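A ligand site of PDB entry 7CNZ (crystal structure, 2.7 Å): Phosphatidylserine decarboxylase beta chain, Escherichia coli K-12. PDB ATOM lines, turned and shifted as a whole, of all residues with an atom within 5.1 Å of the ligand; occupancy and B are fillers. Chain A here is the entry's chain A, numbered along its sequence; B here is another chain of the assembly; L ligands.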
ATOM      1  N   LEU A  13     -16.556   6.891 -26.096  1.00  0.00           N
ATOM      2  CA  LEU A  13     -16.060   5.984 -25.014  1.00  0.00           C
ATOM      3  C   LEU A  13     -17.220   5.532 -24.124  1.00  0.00           C
ATOM      4  O   LEU A  13     -18.145   6.296 -23.885  1.00  0.00           O
ATOM      5  CB  LEU A  13     -14.991   6.703 -24.177  1.00  0.00           C
ATOM      6  CG  LEU A  13     -13.592   6.775 -24.789  1.00  0.00           C
ATOM      7  CD1 LEU A  13     -12.629   7.540 -23.876  1.00  0.00           C
ATOM      8  CD2 LEU A  13     -13.049   5.388 -25.084  1.00  0.00           C
ATOM      9  N   ALA A  22     -11.205   0.223 -14.082  1.00  0.00           N
ATOM     10  CA  ALA A  22     -10.158   0.926 -13.289  1.00  0.00           C
ATOM     11  C   ALA A  22     -10.369   0.668 -11.776  1.00  0.00           C
ATOM     12  O   ALA A  22      -9.379   0.467 -11.051  1.00  0.00           O
ATOM     13  CB  ALA A  22     -10.164   2.402 -13.616  1.00  0.00           C
ATOM     14  N   GLY A  25      -9.388  -2.922 -10.956  1.00  0.00           N
ATOM     15  CA  GLY A  25      -7.907  -2.877 -10.951  1.00  0.00           C
ATOM     16  C   GLY A  25      -7.360  -2.166  -9.734  1.00  0.00           C
ATOM     17  O   GLY A  25      -6.468  -2.724  -9.076  1.00  0.00           O
ATOM     18  N   ALA A  26      -7.880  -0.975  -9.429  1.00  0.00           N
ATOM     19  CA  ALA A  26      -7.325  -0.091  -8.377  1.00  0.00           C
ATOM     20  C   ALA A  26      -7.516  -0.726  -6.989  1.00  0.00           C
ATOM     21  O   ALA A  26      -6.781  -0.329  -6.058  1.00  0.00           O
ATOM     22  CB  ALA A  26      -7.932   1.276  -8.483  1.00  0.00           C
ATOM     23  N   VAL A  37       2.497  -0.053 -11.454  1.00  0.00           N
ATOM     24  CA  VAL A  37       1.473   0.898 -11.975  1.00  0.00           C
ATOM     25  C   VAL A  37       1.519   2.174 -11.110  1.00  0.00           C
ATOM     26  O   VAL A  37       1.447   3.278 -11.686  1.00  0.00           O
ATOM     27  CB  VAL A  37       0.051   0.277 -12.018  1.00  0.00           C
ATOM     28  CG1 VAL A  37      -0.031  -0.890 -12.976  1.00  0.00           C
ATOM     29  CG2 VAL A  37      -0.456  -0.148 -10.656  1.00  0.00           C
ATOM     30  N   PHE A  41       2.662   5.733 -12.752  1.00  0.00           N
ATOM     31  CA  PHE A  41       1.750   6.854 -12.423  1.00  0.00           C
ATOM     32  C   PHE A  41       2.552   7.995 -11.783  1.00  0.00           C
ATOM     33  O   PHE A  41       2.478   9.129 -12.282  1.00  0.00           O
ATOM     34  CB  PHE A  41       0.625   6.376 -11.487  1.00  0.00           C
ATOM     35  CG  PHE A  41      -0.427   7.407 -11.182  1.00  0.00           C
ATOM     36  CD1 PHE A  41      -0.204   8.375 -10.222  1.00  0.00           C
ATOM     37  CD2 PHE A  41      -1.648   7.403 -11.857  1.00  0.00           C
ATOM     38  CE1 PHE A  41      -1.171   9.329  -9.930  1.00  0.00           C
ATOM     39  CE2 PHE A  41      -2.615   8.357 -11.566  1.00  0.00           C
ATOM     40  CZ  PHE A  41      -2.370   9.325 -10.611  1.00  0.00           C
ATOM     41  N   TYR A  45       3.109  11.512 -13.921  1.00  0.00           N
ATOM     42  CA  TYR A  45       2.263  12.623 -13.404  1.00  0.00           C
ATOM     43  C   TYR A  45       3.077  13.572 -12.506  1.00  0.00           C
ATOM     44  O   TYR A  45       2.502  14.602 -12.117  1.00  0.00           O
ATOM     45  CB  TYR A  45       1.022  12.093 -12.672  1.00  0.00           C
ATOM     46  CG  TYR A  45      -0.092  11.655 -13.583  1.00  0.00           C
ATOM     47  CD1 TYR A  45      -0.762  12.565 -14.384  1.00  0.00           C
ATOM     48  CD2 TYR A  45      -0.500  10.333 -13.658  1.00  0.00           C
ATOM     49  CE1 TYR A  45      -1.780  12.186 -15.246  1.00  0.00           C
ATOM     50  CE2 TYR A  45      -1.517   9.929 -14.498  1.00  0.00           C
ATOM     51  CZ  TYR A  45      -2.159  10.852 -15.301  1.00  0.00           C
ATOM     52  OH  TYR A  45      -3.153  10.394 -16.113  1.00  0.00           O
ATOM     53  N   PHE A  63      -3.641   0.109  -5.473  1.00  0.00           N
ATOM     54  CA  PHE A  63      -3.471   1.409  -6.176  1.00  0.00           C
ATOM     55  C   PHE A  63      -4.308   2.481  -5.476  1.00  0.00           C
ATOM     56  O   PHE A  63      -3.757   3.572  -5.207  1.00  0.00           O
ATOM     57  CB  PHE A  63      -3.854   1.359  -7.653  1.00  0.00           C
ATOM     58  CG  PHE A  63      -3.632   2.675  -8.355  1.00  0.00           C
ATOM     59  CD1 PHE A  63      -2.374   3.065  -8.774  1.00  0.00           C
ATOM     60  CD2 PHE A  63      -4.669   3.582  -8.517  1.00  0.00           C
ATOM     61  CE1 PHE A  63      -2.152   4.293  -9.393  1.00  0.00           C
ATOM     62  CE2 PHE A  63      -4.457   4.810  -9.122  1.00  0.00           C
ATOM     63  CZ  PHE A  63      -3.196   5.159  -9.569  1.00  0.00           C
ATOM     64  N   TYR A 137     -10.009  22.419  -9.270  1.00  0.00           N
ATOM     65  CA  TYR A 137      -9.706  21.231 -10.111  1.00  0.00           C
ATOM     66  C   TYR A 137      -8.571  20.437  -9.486  1.00  0.00           C
ATOM     67  O   TYR A 137      -7.476  20.997  -9.350  1.00  0.00           O
ATOM     68  CB  TYR A 137      -9.292  21.630 -11.526  1.00  0.00           C
ATOM     69  CG  TYR A 137      -8.748  20.492 -12.365  1.00  0.00           C
ATOM     70  CD1 TYR A 137      -9.568  19.432 -12.731  1.00  0.00           C
ATOM     71  CD2 TYR A 137      -7.423  20.460 -12.778  1.00  0.00           C
ATOM     72  CE1 TYR A 137      -9.082  18.394 -13.495  1.00  0.00           C
ATOM     73  CE2 TYR A 137      -6.931  19.414 -13.552  1.00  0.00           C
ATOM     74  CZ  TYR A 137      -7.773  18.379 -13.912  1.00  0.00           C
ATOM     75  OH  TYR A 137      -7.333  17.336 -14.673  1.00  0.00           O
ATOM     76  N   LEU A 138      -8.838  19.180  -9.134  1.00  0.00           N
ATOM     77  CA  LEU A 138      -7.821  18.198  -8.654  1.00  0.00           C
ATOM     78  C   LEU A 138      -7.367  17.365  -9.845  1.00  0.00           C
ATOM     79  O   LEU A 138      -8.235  16.680 -10.425  1.00  0.00           O
ATOM     80  CB  LEU A 138      -8.430  17.299  -7.577  1.00  0.00           C
ATOM     81  CG  LEU A 138      -8.796  17.986  -6.258  1.00  0.00           C
ATOM     82  CD1 LEU A 138     -10.137  18.715  -6.351  1.00  0.00           C
ATOM     83  CD2 LEU A 138      -8.830  16.988  -5.116  1.00  0.00           C
ATOM     84  N   SER A 139      -6.078  17.442 -10.217  1.00  0.00           N
ATOM     85  CA  SER A 139      -5.448  16.585 -11.276  1.00  0.00           C
ATOM     86  C   SER A 139      -4.960  15.295 -10.622  1.00  0.00           C
ATOM     87  O   SER A 139      -4.806  15.246  -9.410  1.00  0.00           O
ATOM     88  CB  SER A 139      -4.332  17.302 -11.998  1.00  0.00           C
ATOM     89  OG  SER A 139      -3.073  17.054 -11.360  1.00  0.00           O
ATOM     90  N   PRO A 140      -4.724  14.216 -11.402  1.00  0.00           N
ATOM     91  CA  PRO A 140      -4.296  12.929 -10.833  1.00  0.00           C
ATOM     92  C   PRO A 140      -3.053  13.046  -9.954  1.00  0.00           C
ATOM     93  O   PRO A 140      -2.934  12.317  -8.957  1.00  0.00           O
ATOM     94  CB  PRO A 140      -4.014  12.064 -12.076  1.00  0.00           C
ATOM     95  CG  PRO A 140      -4.887  12.693 -13.172  1.00  0.00           C
ATOM     96  CD  PRO A 140      -4.894  14.174 -12.862  1.00  0.00           C
ATOM     97  N   HIS A 144      -5.954  13.636  -3.242  1.00  0.00           N
ATOM     98  CA  HIS A 144      -7.367  13.502  -3.675  1.00  0.00           C
ATOM     99  C   HIS A 144      -8.336  13.424  -2.481  1.00  0.00           C
ATOM    100  O   HIS A 144      -9.445  12.885  -2.633  1.00  0.00           O
ATOM    101  CB  HIS A 144      -7.488  12.351  -4.674  1.00  0.00           C
ATOM    102  CG  HIS A 144      -7.290  12.807  -6.078  1.00  0.00           C
ATOM    103  ND1 HIS A 144      -8.307  13.416  -6.802  1.00  0.00           N
ATOM    104  CD2 HIS A 144      -6.202  12.783  -6.879  1.00  0.00           C
ATOM    105  CE1 HIS A 144      -7.854  13.739  -7.993  1.00  0.00           C
ATOM    106  NE2 HIS A 144      -6.560  13.353  -8.057  1.00  0.00           N
ATOM    107  N   PHE A 165     -17.967  12.393 -17.416  1.00  0.00           N
ATOM    108  CA  PHE A 165     -17.063  13.137 -18.338  1.00  0.00           C
ATOM    109  C   PHE A 165     -15.739  13.369 -17.632  1.00  0.00           C
ATOM    110  O   PHE A 165     -15.700  13.303 -16.381  1.00  0.00           O
ATOM    111  CB  PHE A 165     -17.699  14.453 -18.785  1.00  0.00           C
ATOM    112  CG  PHE A 165     -18.871  14.289 -19.742  1.00  0.00           C
ATOM    113  CD1 PHE A 165     -18.680  13.764 -21.004  1.00  0.00           C
ATOM    114  CD2 PHE A 165     -20.162  14.624 -19.366  1.00  0.00           C
ATOM    115  CE1 PHE A 165     -19.751  13.590 -21.883  1.00  0.00           C
ATOM    116  CE2 PHE A 165     -21.221  14.450 -20.237  1.00  0.00           C
ATOM    117  CZ  PHE A 165     -21.016  13.933 -21.495  1.00  0.00           C
ATOM    118  N   SER A 166     -14.663  13.629 -18.383  1.00  0.00           N
ATOM    119  CA  SER A 166     -13.427  14.234 -17.834  1.00  0.00           C
ATOM    120  C   SER A 166     -13.785  15.632 -17.337  1.00  0.00           C
ATOM    121  O   SER A 166     -14.788  16.182 -17.826  1.00  0.00           O
ATOM    122  CB  SER A 166     -12.305  14.273 -18.828  1.00  0.00           C
ATOM    123  OG  SER A 166     -11.101  14.770 -18.213  1.00  0.00           O
ATOM    124  N   VAL A 167     -13.023  16.184 -16.390  1.00  0.00           N
ATOM    125  CA  VAL A 167     -13.266  17.530 -15.812  1.00  0.00           C
ATOM    126  C   VAL A 167     -12.032  18.405 -15.950  1.00  0.00           C
ATOM    127  O   VAL A 167     -11.992  19.489 -15.314  1.00  0.00           O
ATOM    128  CB  VAL A 167     -13.747  17.416 -14.344  1.00  0.00           C
ATOM    129  CG1 VAL A 167     -14.888  16.426 -14.193  1.00  0.00           C
ATOM    130  CG2 VAL A 167     -12.617  17.070 -13.404  1.00  0.00           C
ATOM    131  N   ASN A 168     -11.059  18.002 -16.759  1.00  0.00           N
ATOM    132  CA  ASN A 168      -9.869  18.858 -17.078  1.00  0.00           C
ATOM    133  C   ASN A 168     -10.342  20.145 -17.792  1.00  0.00           C
ATOM    134  O   ASN A 168     -11.542  20.210 -18.189  1.00  0.00           O
ATOM    135  CB  ASN A 168      -8.827  18.095 -17.899  1.00  0.00           C
ATOM    136  CG  ASN A 168      -9.351  17.604 -19.228  1.00  0.00           C
ATOM    137  OD1 ASN A 168     -10.283  18.176 -19.780  1.00  0.00           O
ATOM    138  ND2 ASN A 168      -8.762  16.529 -19.735  1.00  0.00           N
ATOM    139  N   ALA A 203     -15.325  12.362 -11.888  1.00  0.00           N
ATOM    140  CA  ALA A 203     -14.877  12.368 -13.290  1.00  0.00           C
ATOM    141  C   ALA A 203     -14.687  10.932 -13.759  1.00  0.00           C
ATOM    142  O   ALA A 203     -14.835  10.029 -12.929  1.00  0.00           O
ATOM    143  CB  ALA A 203     -13.596  13.168 -13.397  1.00  0.00           C
ATOM    144  N   THR A 204     -14.398  10.730 -15.040  1.00  0.00           N
ATOM    145  CA  THR A 204     -14.061   9.401 -15.628  1.00  0.00           C
ATOM    146  C   THR A 204     -12.943   8.775 -14.790  1.00  0.00           C
ATOM    147  O   THR A 204     -12.029   9.524 -14.395  1.00  0.00           O
ATOM    148  CB  THR A 204     -13.615   9.535 -17.085  1.00  0.00           C
ATOM    149  OG1 THR A 204     -14.188  10.716 -17.647  1.00  0.00           O
ATOM    150  CG2 THR A 204     -13.991   8.317 -17.886  1.00  0.00           C
ATOM    151  N   ILE A 205     -13.025   7.461 -14.542  1.00  0.00           N
ATOM    152  CA  ILE A 205     -12.019   6.670 -13.760  1.00  0.00           C
ATOM    153  C   ILE A 205     -12.143   7.053 -12.264  1.00  0.00           C
ATOM    154  O   ILE A 205     -12.473   6.162 -11.435  1.00  0.00           O
ATOM    155  CB  ILE A 205     -10.583   6.887 -14.299  1.00  0.00           C
ATOM    156  CG1 ILE A 205     -10.460   6.622 -15.800  1.00  0.00           C
ATOM    157  CG2 ILE A 205      -9.568   6.063 -13.505  1.00  0.00           C
ATOM    158  CD1 ILE A 205     -10.830   5.226 -16.212  1.00  0.00           C
ATOM    159  N   VAL A 206     -11.894   8.318 -11.942  1.00  0.00           N
ATOM    160  CA  VAL A 206     -11.945   8.864 -10.559  1.00  0.00           C
ATOM    161  C   VAL A 206     -13.402   9.263 -10.278  1.00  0.00           C
ATOM    162  O   VAL A 206     -13.706  10.470 -10.230  1.00  0.00           O
ATOM    163  CB  VAL A 206     -10.968  10.054 -10.459  1.00  0.00           C
ATOM    164  CG1 VAL A 206     -10.851  10.599  -9.042  1.00  0.00           C
ATOM    165  CG2 VAL A 206      -9.600   9.650 -10.995  1.00  0.00           C
ATOM    166  N   LEU A 252     -10.809   5.631  -7.366  1.00  0.00           N
ATOM    167  CA  LEU A 252     -11.151   5.000  -8.663  1.00  0.00           C
ATOM    168  C   LEU A 252     -12.278   4.004  -8.424  1.00  0.00           C
ATOM    169  O   LEU A 252     -12.238   3.286  -7.377  1.00  0.00           O
ATOM    170  CB  LEU A 252      -9.895   4.328  -9.244  1.00  0.00           C
ATOM    171  CG  LEU A 252      -8.904   5.292  -9.892  1.00  0.00           C
ATOM    172  CD1 LEU A 252      -8.182   6.131  -8.843  1.00  0.00           C
ATOM    173  CD2 LEU A 252      -7.915   4.543 -10.771  1.00  0.00           C
ATOM    174  C   PYR B   1     -11.898  16.881  -9.337  1.00  0.00           C
ATOM    175  O   PYR B   1     -11.106  17.615  -9.956  1.00  0.00           O
ATOM    176  CA  PYR B   1     -11.450  15.463  -9.020  1.00  0.00           C
ATOM    177  CB  PYR B   1     -12.642  14.520  -8.932  1.00  0.00           C
ATOM    178  N   THR B   2     -13.089  17.294  -8.831  1.00  0.00           N
ATOM    179  CA  THR B   2     -13.446  18.706  -8.800  1.00  0.00           C
ATOM    180  C   THR B   2     -14.248  18.989  -7.526  1.00  0.00           C
ATOM    181  O   THR B   2     -15.100  18.164  -7.144  1.00  0.00           O
ATOM    182  CB  THR B   2     -14.241  19.143 -10.038  1.00  0.00           C
ATOM    183  OG1 THR B   2     -13.348  19.328 -11.133  1.00  0.00           O
ATOM    184  CG2 THR B   2     -14.987  20.440  -9.840  1.00  0.00           C
HETATM  185  O1  LIG L   1      -9.022  15.234 -15.838  1.00  0.00           O
HETATM  186  O2  LIG L   1     -11.081  14.134 -15.570  1.00  0.00           O
HETATM  187  P1  LIG L   1      -9.726  14.250 -14.923  1.00  0.00           P
HETATM  188  O3  LIG L   1      -9.051  12.790 -14.829  1.00  0.00           O
HETATM  189  C1  LIG L   1      -9.773  11.564 -14.692  1.00  0.00           C
HETATM  190  C2  LIG L   1      -9.281  10.513 -15.721  1.00  0.00           C
HETATM  191  C3  LIG L   1      -9.794  10.874 -17.115  1.00  0.00           C
HETATM  192  O4  LIG L   1      -9.845   9.693 -17.896  1.00  0.00           O
HETATM  193  C4  LIG L   1      -9.711   9.716 -19.344  1.00  0.00           C
HETATM  194  O5  LIG L   1      -9.300  10.767 -19.771  1.00  0.00           O
HETATM  195  C5  LIG L   1     -10.055   8.543 -20.262  1.00  0.00           C
HETATM  196  O6  LIG L   1      -7.841  10.401 -15.750  1.00  0.00           O
HETATM  197  C6  LIG L   1      -7.299   9.307 -14.982  1.00  0.00           C
HETATM  198  O7  LIG L   1      -7.934   8.870 -14.051  1.00  0.00           O
HETATM  199  C7  LIG L   1      -5.962   8.732 -15.368  1.00  0.00           C
HETATM  200  C8  LIG L   1      -5.328   7.862 -14.271  1.00  0.00           C
HETATM  201  C9  LIG L   1      -4.712   6.594 -14.872  1.00  0.00           C
HETATM  202  C10 LIG L   1      -5.539   5.337 -14.648  1.00  0.00           C
HETATM  203  C11 LIG L   1      -5.174   4.636 -13.348  1.00  0.00           C
HETATM  204  C12 LIG L   1      -4.717   3.189 -13.571  1.00  0.00           C
HETATM  205  C13 LIG L   1      -5.723   2.143 -13.064  1.00  0.00           C
HETATM  206  C14 LIG L   1      -5.567   1.755 -11.584  1.00  0.00           C
HETATM  207  C15 LIG L   1      -5.391   0.258 -11.350  1.00  0.00           C
HETATM  208  O8  LIG L   1      -9.637  14.866 -13.417  1.00  0.00           O
HETATM  209  C16 LIG L   1      -9.920  14.111 -12.232  1.00  0.00           C
HETATM  210  C17 LIG L   1     -10.978  14.749 -11.321  1.00  0.00           C
HETATM  211  N1  LIG L   1     -10.451  14.895  -9.957  1.00  0.00           N
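C of Gly 25 touches C15 of the ligand, 3.5 Å away. Ala 26 touches the ligand. Phe 41 touches the ligand (CE2 to C8, 3.9 Å). Tyr 45 touches the ligand. Phe 63 touches the ligand (CD2 to C14, 3.7 Å). His 144 touches the ligand (CE1 to N1, 3.5 Å). Asn 168 touches the ligand. Ala 203 touches the ligand (CB to O2, 3.5 Å). Thr 204 touches the ligand (O to C1, 3.1 Å). Ile 205 touches the ligand (CG2 to O7, 3.3 Å). Val 206 touches the ligand. Leu 252 touches the ligand (CD2 to C14, 3.7 Å). Thr 2 of chain B touches the ligand. Hydrophobic or aromatic side chains that line the ligand: Ala 26, Phe 41, Phe 63, Tyr 137, Leu 138, His 144, Val 167, Ala 203, Ile 205, Val 206 and Leu 252. The nearest printed residue that does not touch the ligand is Ala 22 (4.005 Å).
O of PYR 1 of chain B lies close to N1 of the ligand, at 2.8 Å. O2 of the ligand is in hydrogen-bond range of OG of Ser 166, 2.7 Å away. A nitrogen (N1) of the ligand sits at hydrogen-bond distance from the backbone carbonyl oxygen of Leu 138 (2.9 Å). The side-chain hydroxyl of Tyr 137 is in hydrogen-bond range of an oxygen (O1) of the ligand (2.9 Å). The backbone NH (N) of Val 167 sits at hydrogen-bond distance from an oxygen (O2) of the ligand (2.9 Å).
O of PYR 1 of chain B sits at hydrogen-bond distance from the backbone NH (N) of Leu 138 (2.9 Å). The backbone NH (N) of Ser 166 is in hydrogen-bond range of the side-chain hydroxyl (OG1) of Thr 204 (3.0 Å). ND2 of Asn 168 lies within hydrogen-bond range of OG of Ser 166 (3.3 Å). The backbone carbonyl oxygen of Phe 165 is in hydrogen-bond range of the backbone NH of Thr 204 (3.2 Å). The backbone carbonyl oxygen (O) of Ala 26 is in hydrogen-bond range of the backbone NH (N) of Phe 63, 3.2 Å away. A ring nitrogen (NE2) of His 144 sits at hydrogen-bond distance from the backbone carbonyl oxygen (O) of Ser 139 (2.9 Å).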
